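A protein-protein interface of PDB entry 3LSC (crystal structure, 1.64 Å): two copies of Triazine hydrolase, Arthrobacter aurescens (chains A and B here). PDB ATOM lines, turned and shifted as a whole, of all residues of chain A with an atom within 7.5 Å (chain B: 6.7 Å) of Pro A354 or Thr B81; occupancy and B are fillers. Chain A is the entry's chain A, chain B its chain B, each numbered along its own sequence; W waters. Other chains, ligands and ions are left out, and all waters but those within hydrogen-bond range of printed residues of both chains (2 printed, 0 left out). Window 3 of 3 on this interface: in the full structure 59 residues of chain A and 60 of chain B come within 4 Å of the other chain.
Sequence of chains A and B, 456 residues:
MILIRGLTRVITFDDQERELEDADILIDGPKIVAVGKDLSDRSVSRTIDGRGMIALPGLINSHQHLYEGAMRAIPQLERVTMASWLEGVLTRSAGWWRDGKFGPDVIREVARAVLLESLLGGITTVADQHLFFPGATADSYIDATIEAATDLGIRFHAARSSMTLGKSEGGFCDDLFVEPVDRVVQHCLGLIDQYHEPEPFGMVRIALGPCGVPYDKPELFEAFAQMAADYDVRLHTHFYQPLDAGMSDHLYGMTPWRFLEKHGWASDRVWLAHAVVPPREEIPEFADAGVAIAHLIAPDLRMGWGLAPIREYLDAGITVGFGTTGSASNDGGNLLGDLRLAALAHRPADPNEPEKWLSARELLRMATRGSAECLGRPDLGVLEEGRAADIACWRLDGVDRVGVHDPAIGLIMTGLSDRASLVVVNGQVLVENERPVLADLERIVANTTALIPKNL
The guanidinium group (NH1) of Arg B79 sits at hydrogen-bond distance from the backbone carbonyl oxygen (O) of Trp A357, 2.9 Å away. The guanidinium group of Arg A347 is in hydrogen-bond range of the backbone carbonyl oxygen of Arg B302, at 2.9 Å. The backbone carbonyl oxygen of Glu A355 sits at hydrogen-bond distance from the guanidinium group of Arg B79 (3.5 Å).
O of Arg A347 sits at hydrogen-bond distance from NE1 of Trp A357, 3.2 Å away. NE1 of Trp A357 is in hydrogen-bond range of O of Asp A350. NH2 of Arg A311 sits at hydrogen-bond distance from O of Trp A357, at 3.0 Å. NE of Arg A311 lies within hydrogen-bond range of O of Lys A356.
NH1 of Arg B79 touches NH2 of Arg A311, at 3.9 Å. O of Pro A351 touches CG2 of Thr B81, 3.96 Å away. CB of Pro A354 touches O of Arg B79 (3.4 Å). Pro A354 touches Val B80. CG2 of Thr B81 touches CD of Pro A354 (3.98 Å). Trp A357 touches Val B80. Arg B302 touches Trp A357 (O to CZ3, 3.5 Å). Met B303 touches Trp A357 (O to CH2, 3.9 Å). Arg B79 touches Ser A359.
Of the printed residues of chain B, Pro A354 touches Arg B79, Val B80 and Thr B81. Of chain A, only Pro A351 (3.96 Å) and Pro A354 (3.98 Å) come within 4 Å of Thr B81. Printed residues of chain B within 4 Å of Glu A355: Arg B79 (3.5 Å). Printed residues of chain A within 4 Å of Arg B302: Arg A347 and Trp A357. Printed residues of chain A within 4 Å of Met B303: Trp A357 (3.9 Å). Printed residues of chain A within 4 Å of Arg B79: Arg A311, Pro A354, Glu A355, Trp A357 and Ser A359. Ala B83 touches none of the printed residues of chain A. Leu A358 touches none of the printed residues of chain B. The nearest printed residue of chain B that does not touch Pro A354 is Ser B84 (6.6 Å). The nearest residue of chain A that does not touch Thr B81 is Asn A352 (4.5 Å).
Water W1 lies within hydrogen-bond range of the backbone carbonyl oxygen of Met B303 (2.6 Å) and the backbone carbonyl oxygen of Pro A351 (2.7 Å). Water W2 lies within hydrogen-bond range of O of Arg B302 (2.7 Å), O of Val B80 (2.7 Å) and NH1 of Arg A347 (3.1 Å).
Hydrophobic or aromatic side chains of chain A that line the printed part of chain B: Pro A354 and Trp A357. Among the printed residues, 12 pairs touch across the chains.
No position is printed for both chains.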
ATOM      1  N   ARG A 311      -0.671 -12.044 -15.288  1.00  0.00           N
ATOM      2  CA  ARG A 311      -1.049 -13.347 -15.827  1.00  0.00           C
ATOM      3  C   ARG A 311      -2.330 -13.215 -16.647  1.00  0.00           C
ATOM      4  O   ARG A 311      -2.448 -13.783 -17.731  1.00  0.00           O
ATOM      5  CB  ARG A 311      -1.244 -14.368 -14.707  1.00  0.00           C
ATOM      6  CG  ARG A 311      -1.756 -15.721 -15.182  1.00  0.00           C
ATOM      7  CD  ARG A 311      -0.863 -16.331 -16.258  1.00  0.00           C
ATOM      8  NE  ARG A 311       0.485 -16.623 -15.763  1.00  0.00           N
ATOM      9  CZ  ARG A 311       1.560 -16.738 -16.539  1.00  0.00           C
ATOM     10  NH1 ARG A 311       1.458 -16.617 -17.852  1.00  0.00           N
ATOM     11  NH2 ARG A 311       2.744 -16.997 -15.991  1.00  0.00           N
ATOM     12  N   ARG A 347       4.362 -14.257  -6.602  1.00  0.00           N
ATOM     13  CA  ARG A 347       4.094 -15.630  -6.190  1.00  0.00           C
ATOM     14  C   ARG A 347       3.088 -15.797  -5.042  1.00  0.00           C
ATOM     15  O   ARG A 347       2.190 -16.634  -5.132  1.00  0.00           O
ATOM     16  CB  ARG A 347       5.411 -16.347  -5.895  1.00  0.00           C
ATOM     17  CG  ARG A 347       6.345 -16.357  -7.099  1.00  0.00           C
ATOM     18  CD  ARG A 347       7.671 -17.061  -6.785  1.00  0.00           C
ATOM     19  NE  ARG A 347       8.518 -17.171  -7.973  1.00  0.00           N
ATOM     20  CZ  ARG A 347       9.310 -18.203  -8.250  1.00  0.00           C
ATOM     21  NH1 ARG A 347       9.384 -19.244  -7.421  1.00  0.00           N
ATOM     22  NH2 ARG A 347      10.038 -18.198  -9.359  1.00  0.00           N
ATOM     23  N   ASP A 350      -0.762 -16.351  -5.522  1.00  0.00           N
ATOM     24  CA  ASP A 350      -1.298 -17.635  -5.969  1.00  0.00           C
ATOM     25  C   ASP A 350      -0.503 -18.784  -5.340  1.00  0.00           C
ATOM     26  O   ASP A 350       0.169 -19.535  -6.038  1.00  0.00           O
ATOM     27  CB  ASP A 350      -1.276 -17.720  -7.501  1.00  0.00           C
ATOM     28  CG  ASP A 350      -2.246 -16.748  -8.154  1.00  0.00           C
ATOM     29  OD1 ASP A 350      -3.473 -16.894  -7.958  1.00  0.00           O
ATOM     30  OD2 ASP A 350      -1.783 -15.831  -8.866  1.00  0.00           O
ATOM     31  N   PRO A 351      -0.597 -18.913  -4.010  1.00  0.00           N
ATOM     32  CA  PRO A 351       0.226 -19.820  -3.196  1.00  0.00           C
ATOM     33  C   PRO A 351       0.206 -21.263  -3.688  1.00  0.00           C
ATOM     34  O   PRO A 351       1.223 -21.966  -3.557  1.00  0.00           O
ATOM     35  CB  PRO A 351      -0.426 -19.748  -1.814  1.00  0.00           C
ATOM     36  CG  PRO A 351      -1.234 -18.523  -1.807  1.00  0.00           C
ATOM     37  CD  PRO A 351      -1.632 -18.233  -3.215  1.00  0.00           C
ATOM     38  N   ASN A 352      -0.925 -21.705  -4.232  1.00  0.00           N
ATOM     39  CA  ASN A 352      -1.080 -23.115  -4.614  1.00  0.00           C
ATOM     40  C   ASN A 352      -1.140 -23.378  -6.121  1.00  0.00           C
ATOM     41  O   ASN A 352      -1.403 -24.505  -6.553  1.00  0.00           O
ATOM     42  CB  ASN A 352      -2.316 -23.718  -3.933  1.00  0.00           C
ATOM     43  CG  ASN A 352      -2.392 -23.384  -2.456  1.00  0.00           C
ATOM     44  OD1 ASN A 352      -3.370 -22.794  -1.991  1.00  0.00           O
ATOM     45  ND2 ASN A 352      -1.358 -23.754  -1.709  1.00  0.00           N
ATOM     46  N   GLU A 353      -0.881 -22.349  -6.920  1.00  0.00           N
ATOM     47  CA  GLU A 353      -0.939 -22.478  -8.371  1.00  0.00           C
ATOM     48  C   GLU A 353       0.298 -21.871  -9.024  1.00  0.00           C
ATOM     49  O   GLU A 353       0.210 -20.816  -9.657  1.00  0.00           O
ATOM     50  CB  GLU A 353      -2.194 -21.782  -8.922  1.00  0.00           C
ATOM     51  CG  GLU A 353      -3.502 -22.410  -8.464  1.00  0.00           C
ATOM     52  CD  GLU A 353      -4.704 -21.866  -9.217  1.00  0.00           C
ATOM     53  OE1 GLU A 353      -5.363 -20.937  -8.703  1.00  0.00           O
ATOM     54  OE2 GLU A 353      -4.990 -22.370 -10.325  1.00  0.00           O
ATOM     55  N   PRO A 354       1.451 -22.539  -8.876  1.00  0.00           N
ATOM     56  CA  PRO A 354       2.729 -22.014  -9.369  1.00  0.00           C
ATOM     57  C   PRO A 354       2.754 -21.821 -10.879  1.00  0.00           C
ATOM     58  O   PRO A 354       3.550 -21.026 -11.369  1.00  0.00           O
ATOM     59  CB  PRO A 354       3.740 -23.090  -8.956  1.00  0.00           C
ATOM     60  CG  PRO A 354       2.911 -24.336  -8.732  1.00  0.00           C
ATOM     61  CD  PRO A 354       1.613 -23.830  -8.186  1.00  0.00           C
ATOM     62  N   GLU A 355       1.903 -22.536 -11.604  1.00  0.00           N
ATOM     63  CA  GLU A 355       1.816 -22.358 -13.049  1.00  0.00           C
ATOM     64  C   GLU A 355       1.363 -20.933 -13.426  1.00  0.00           C
ATOM     65  O   GLU A 355       1.580 -20.472 -14.548  1.00  0.00           O
ATOM     66  CB  GLU A 355       0.892 -23.417 -13.666  1.00  0.00           C
ATOM     67  CG  GLU A 355      -0.590 -23.288 -13.283  1.00  0.00           C
ATOM     68  CD  GLU A 355      -0.946 -23.842 -11.892  1.00  0.00           C
ATOM     69  OE1 GLU A 355      -0.096 -24.479 -11.223  1.00  0.00           O
ATOM     70  OE2 GLU A 355      -2.113 -23.637 -11.476  1.00  0.00           O
ATOM     71  N   LYS A 356       0.753 -20.235 -12.476  1.00  0.00           N
ATOM     72  CA  LYS A 356       0.305 -18.866 -12.697  1.00  0.00           C
ATOM     73  C   LYS A 356       1.437 -17.852 -12.517  1.00  0.00           C
ATOM     74  O   LYS A 356       1.372 -16.743 -13.052  1.00  0.00           O
ATOM     75  CB  LYS A 356      -0.853 -18.512 -11.760  1.00  0.00           C
ATOM     76  CG  LYS A 356      -2.164 -19.190 -12.129  1.00  0.00           C
ATOM     77  CD  LYS A 356      -3.312 -18.713 -11.259  1.00  0.00           C
ATOM     78  CE  LYS A 356      -4.613 -19.434 -11.614  1.00  0.00           C
ATOM     79  NZ  LYS A 356      -5.754 -18.974 -10.773  1.00  0.00           N
ATOM     80  N   TRP A 357       2.457 -18.226 -11.752  1.00  0.00           N
ATOM     81  CA  TRP A 357       3.550 -17.296 -11.469  1.00  0.00           C
ATOM     82  C   TRP A 357       4.283 -16.937 -12.757  1.00  0.00           C
ATOM     83  O   TRP A 357       4.417 -17.765 -13.657  1.00  0.00           O
ATOM     84  CB  TRP A 357       4.543 -17.905 -10.473  1.00  0.00           C
ATOM     85  CG  TRP A 357       3.940 -18.404  -9.190  1.00  0.00           C
ATOM     86  CD1 TRP A 357       2.683 -18.166  -8.714  1.00  0.00           C
ATOM     87  CD2 TRP A 357       4.587 -19.235  -8.215  1.00  0.00           C
ATOM     88  NE1 TRP A 357       2.507 -18.798  -7.499  1.00  0.00           N
ATOM     89  CE2 TRP A 357       3.663 -19.460  -7.176  1.00  0.00           C
ATOM     90  CE3 TRP A 357       5.860 -19.799  -8.120  1.00  0.00           C
ATOM     91  CZ2 TRP A 357       3.970 -20.236  -6.058  1.00  0.00           C
ATOM     92  CZ3 TRP A 357       6.161 -20.571  -7.010  1.00  0.00           C
ATOM     93  CH2 TRP A 357       5.220 -20.778  -5.993  1.00  0.00           C
ATOM     94  N   LEU A 358       4.776 -15.706 -12.848  1.00  0.00           N
ATOM     95  CA  LEU A 358       5.518 -15.295 -14.033  1.00  0.00           C
ATOM     96  C   LEU A 358       6.885 -15.972 -14.063  1.00  0.00           C
ATOM     97  O   LEU A 358       7.593 -16.000 -13.054  1.00  0.00           O
ATOM     98  CB  LEU A 358       5.697 -13.778 -14.056  1.00  0.00           C
ATOM     99  CG  LEU A 358       4.416 -12.967 -13.877  1.00  0.00           C
ATOM    100  CD1 LEU A 358       4.739 -11.485 -13.880  1.00  0.00           C
ATOM    101  CD2 LEU A 358       3.412 -13.313 -14.961  1.00  0.00           C
ATOM    102  N   SER A 359       7.263 -16.505 -15.216  1.00  0.00           N
ATOM    103  CA  SER A 359       8.564 -17.166 -15.340  1.00  0.00           C
ATOM    104  C   SER A 359       9.674 -16.193 -15.716  1.00  0.00           C
ATOM    105  O   SER A 359       9.416 -15.094 -16.233  1.00  0.00           O
ATOM    106  CB  SER A 359       8.512 -18.295 -16.377  1.00  0.00           C
ATOM    107  OG  SER A 359       8.441 -17.772 -17.690  1.00  0.00           O
ATOM    108  N   ARG B  79       9.235 -22.804 -10.568  1.00  0.00           N
ATOM    109  CA  ARG B  79       7.918 -22.470 -10.038  1.00  0.00           C
ATOM    110  C   ARG B  79       7.296 -23.707  -9.400  1.00  0.00           C
ATOM    111  O   ARG B  79       6.590 -24.462 -10.063  1.00  0.00           O
ATOM    112  CB  ARG B  79       7.009 -21.941 -11.157  1.00  0.00           C
ATOM    113  CG  ARG B  79       7.482 -20.633 -11.786  1.00  0.00           C
ATOM    114  CD  ARG B  79       6.564 -20.195 -12.925  1.00  0.00           C
ATOM    115  NE  ARG B  79       6.752 -21.008 -14.123  1.00  0.00           N
ATOM    116  CZ  ARG B  79       5.983 -20.951 -15.204  1.00  0.00           C
ATOM    117  NH1 ARG B  79       4.950 -20.113 -15.257  1.00  0.00           N
ATOM    118  NH2 ARG B  79       6.249 -21.732 -16.239  1.00  0.00           N
ATOM    119  N   VAL B  80       7.562 -23.904  -8.113  1.00  0.00           N
ATOM    120  CA  VAL B  80       7.058 -25.069  -7.389  1.00  0.00           C
ATOM    121  C   VAL B  80       6.632 -24.670  -5.985  1.00  0.00           C
ATOM    122  O   VAL B  80       7.155 -23.706  -5.417  1.00  0.00           O
ATOM    123  CB  VAL B  80       8.121 -26.189  -7.288  1.00  0.00           C
ATOM    124  CG1 VAL B  80       8.356 -26.832  -8.648  1.00  0.00           C
ATOM    125  CG2 VAL B  80       9.415 -25.652  -6.702  1.00  0.00           C
ATOM    126  N   THR B  81       5.670 -25.407  -5.437  1.00  0.00           N
ATOM    127  CA  THR B  81       5.285 -25.269  -4.037  1.00  0.00           C
ATOM    128  C   THR B  81       6.313 -25.988  -3.165  1.00  0.00           C
ATOM    129  O   THR B  81       7.158 -26.720  -3.671  1.00  0.00           O
ATOM    130  CB  THR B  81       3.911 -25.912  -3.773  1.00  0.00           C
ATOM    131  OG1 THR B  81       4.016 -27.335  -3.930  1.00  0.00           O
ATOM    132  CG2 THR B  81       2.865 -25.371  -4.738  1.00  0.00           C
ATOM    133  N   MET B  82       6.232 -25.783  -1.855  1.00  0.00           N
ATOM    134  CA  MET B  82       7.179 -26.410  -0.935  1.00  0.00           C
ATOM    135  C   MET B  82       7.296 -27.920  -1.141  1.00  0.00           C
ATOM    136  O   MET B  82       8.400 -28.457  -1.247  1.00  0.00           O
ATOM    137  CB  MET B  82       6.808 -26.100   0.518  1.00  0.00           C
ATOM    138  CG  MET B  82       7.810 -26.644   1.539  1.00  0.00           C
ATOM    139  SD  MET B  82       9.506 -26.104   1.199  1.00  0.00           S
ATOM    140  CE  MET B  82      10.339 -26.576   2.714  1.00  0.00           C
ATOM    141  N   ALA B  83       6.157 -28.604  -1.198  1.00  0.00           N
ATOM    142  CA  ALA B  83       6.150 -30.057  -1.340  1.00  0.00           C
ATOM    143  C   ALA B  83       6.947 -30.530  -2.552  1.00  0.00           C
ATOM    144  O   ALA B  83       7.799 -31.420  -2.438  1.00  0.00           O
ATOM    145  CB  ALA B  83       4.719 -30.581  -1.404  1.00  0.00           C
ATOM    146  N   SER B  84       6.663 -29.942  -3.712  1.00  0.00           N
ATOM    147  CA  SER B  84       7.352 -30.299  -4.945  1.00  0.00           C
ATOM    148  C   SER B  84       8.821 -29.901  -4.853  1.00  0.00           C
ATOM    149  O   SER B  84       9.691 -30.572  -5.410  1.00  0.00           O
ATOM    150  CB  SER B  84       6.715 -29.596  -6.150  1.00  0.00           C
ATOM    151  OG  SER B  84       5.340 -29.921  -6.292  1.00  0.00           O
ATOM    152  N   TRP B  85       9.084 -28.794  -4.163  1.00  0.00           N
ATOM    153  CA  TRP B  85      10.440 -28.284  -4.013  1.00  0.00           C
ATOM    154  C   TRP B  85      11.281 -29.263  -3.196  1.00  0.00           C
ATOM    155  O   TRP B  85      12.371 -29.649  -3.608  1.00  0.00           O
ATOM    156  CB  TRP B  85      10.434 -26.911  -3.330  1.00  0.00           C
ATOM    157  CG  TRP B  85      11.795 -26.290  -3.226  1.00  0.00           C
ATOM    158  CD1 TRP B  85      12.414 -25.512  -4.163  1.00  0.00           C
ATOM    159  CD2 TRP B  85      12.703 -26.387  -2.122  1.00  0.00           C
ATOM    160  NE1 TRP B  85      13.656 -25.125  -3.711  1.00  0.00           N
ATOM    161  CE2 TRP B  85      13.857 -25.651  -2.461  1.00  0.00           C
ATOM    162  CE3 TRP B  85      12.659 -27.039  -0.884  1.00  0.00           C
ATOM    163  CZ2 TRP B  85      14.957 -25.541  -1.603  1.00  0.00           C
ATOM    164  CZ3 TRP B  85      13.743 -26.925  -0.036  1.00  0.00           C
ATOM    165  CH2 TRP B  85      14.879 -26.182  -0.398  1.00  0.00           C
ATOM    166  N   LEU B  86      10.762 -29.657  -2.038  1.00  0.00           N
ATOM    167  CA  LEU B  86      11.475 -30.566  -1.153  1.00  0.00           C
ATOM    168  C   LEU B  86      11.729 -31.888  -1.872  1.00  0.00           C
ATOM    169  O   LEU B  86      12.828 -32.445  -1.809  1.00  0.00           O
ATOM    170  CB  LEU B  86      10.672 -30.781   0.133  1.00  0.00           C
ATOM    171  CG  LEU B  86      11.389 -31.362   1.350  1.00  0.00           C
ATOM    172  CD1 LEU B  86      12.650 -30.567   1.666  1.00  0.00           C
ATOM    173  CD2 LEU B  86      10.444 -31.382   2.546  1.00  0.00           C
ATOM    174  N   ARG B 302       9.639 -16.696  -2.838  1.00  0.00           N
ATOM    175  CA  ARG B 302       9.868 -17.702  -3.865  1.00  0.00           C
ATOM    176  C   ARG B 302       8.943 -18.905  -3.698  1.00  0.00           C
ATOM    177  O   ARG B 302       8.538 -19.527  -4.681  1.00  0.00           O
ATOM    178  CB  ARG B 302      11.316 -18.184  -3.823  1.00  0.00           C
ATOM    179  CG  ARG B 302      11.708 -19.043  -5.010  1.00  0.00           C
ATOM    180  CD  ARG B 302      12.859 -19.946  -4.639  1.00  0.00           C
ATOM    181  NE  ARG B 302      13.582 -20.474  -5.796  1.00  0.00           N
ATOM    182  CZ  ARG B 302      13.174 -21.497  -6.545  1.00  0.00           C
ATOM    183  NH1 ARG B 302      12.010 -22.093  -6.305  1.00  0.00           N
ATOM    184  NH2 ARG B 302      13.921 -21.905  -7.561  1.00  0.00           N
ATOM    185  N   MET B 303       8.626 -19.237  -2.450  1.00  0.00           N
ATOM    186  CA  MET B 303       7.769 -20.382  -2.164  1.00  0.00           C
ATOM    187  C   MET B 303       6.300 -20.017  -2.241  1.00  0.00           C
ATOM    188  O   MET B 303       5.430 -20.887  -2.149  1.00  0.00           O
ATOM    189  CB  MET B 303       8.070 -20.950  -0.775  1.00  0.00           C
ATOM    190  CG  MET B 303       9.414 -21.618  -0.670  1.00  0.00           C
ATOM    191  SD  MET B 303       9.526 -23.004  -1.819  1.00  0.00           S
ATOM    192  CE  MET B 303      10.648 -22.320  -3.009  1.00  0.00           C
ATOM    193  N   TRP B 305       4.896 -18.062  -0.010  1.00  0.00           N
ATOM    194  CA  TRP B 305       4.467 -17.988   1.389  1.00  0.00           C
ATOM    195  C   TRP B 305       3.967 -16.624   1.839  1.00  0.00           C
ATOM    196  O   TRP B 305       3.034 -16.537   2.635  1.00  0.00           O
ATOM    197  CB  TRP B 305       5.598 -18.427   2.321  1.00  0.00           C
ATOM    198  CG  TRP B 305       5.958 -19.874   2.194  1.00  0.00           C
ATOM    199  CD1 TRP B 305       5.258 -20.835   1.525  1.00  0.00           C
ATOM    200  CD2 TRP B 305       7.110 -20.521   2.740  1.00  0.00           C
ATOM    201  NE1 TRP B 305       5.904 -22.045   1.624  1.00  0.00           N
ATOM    202  CE2 TRP B 305       7.046 -21.878   2.364  1.00  0.00           C
ATOM    203  CE3 TRP B 305       8.198 -20.083   3.506  1.00  0.00           C
ATOM    204  CZ2 TRP B 305       8.021 -22.811   2.740  1.00  0.00           C
ATOM    205  CZ3 TRP B 305       9.168 -21.014   3.878  1.00  0.00           C
ATOM    206  CH2 TRP B 305       9.072 -22.358   3.489  1.00  0.00           C
HETATM  207  O   HOH W   1       3.045 -21.785  -1.566  1.00  0.00           O
HETATM  208  O   HOH W   2       9.142 -21.880  -5.885  1.00  0.00           O
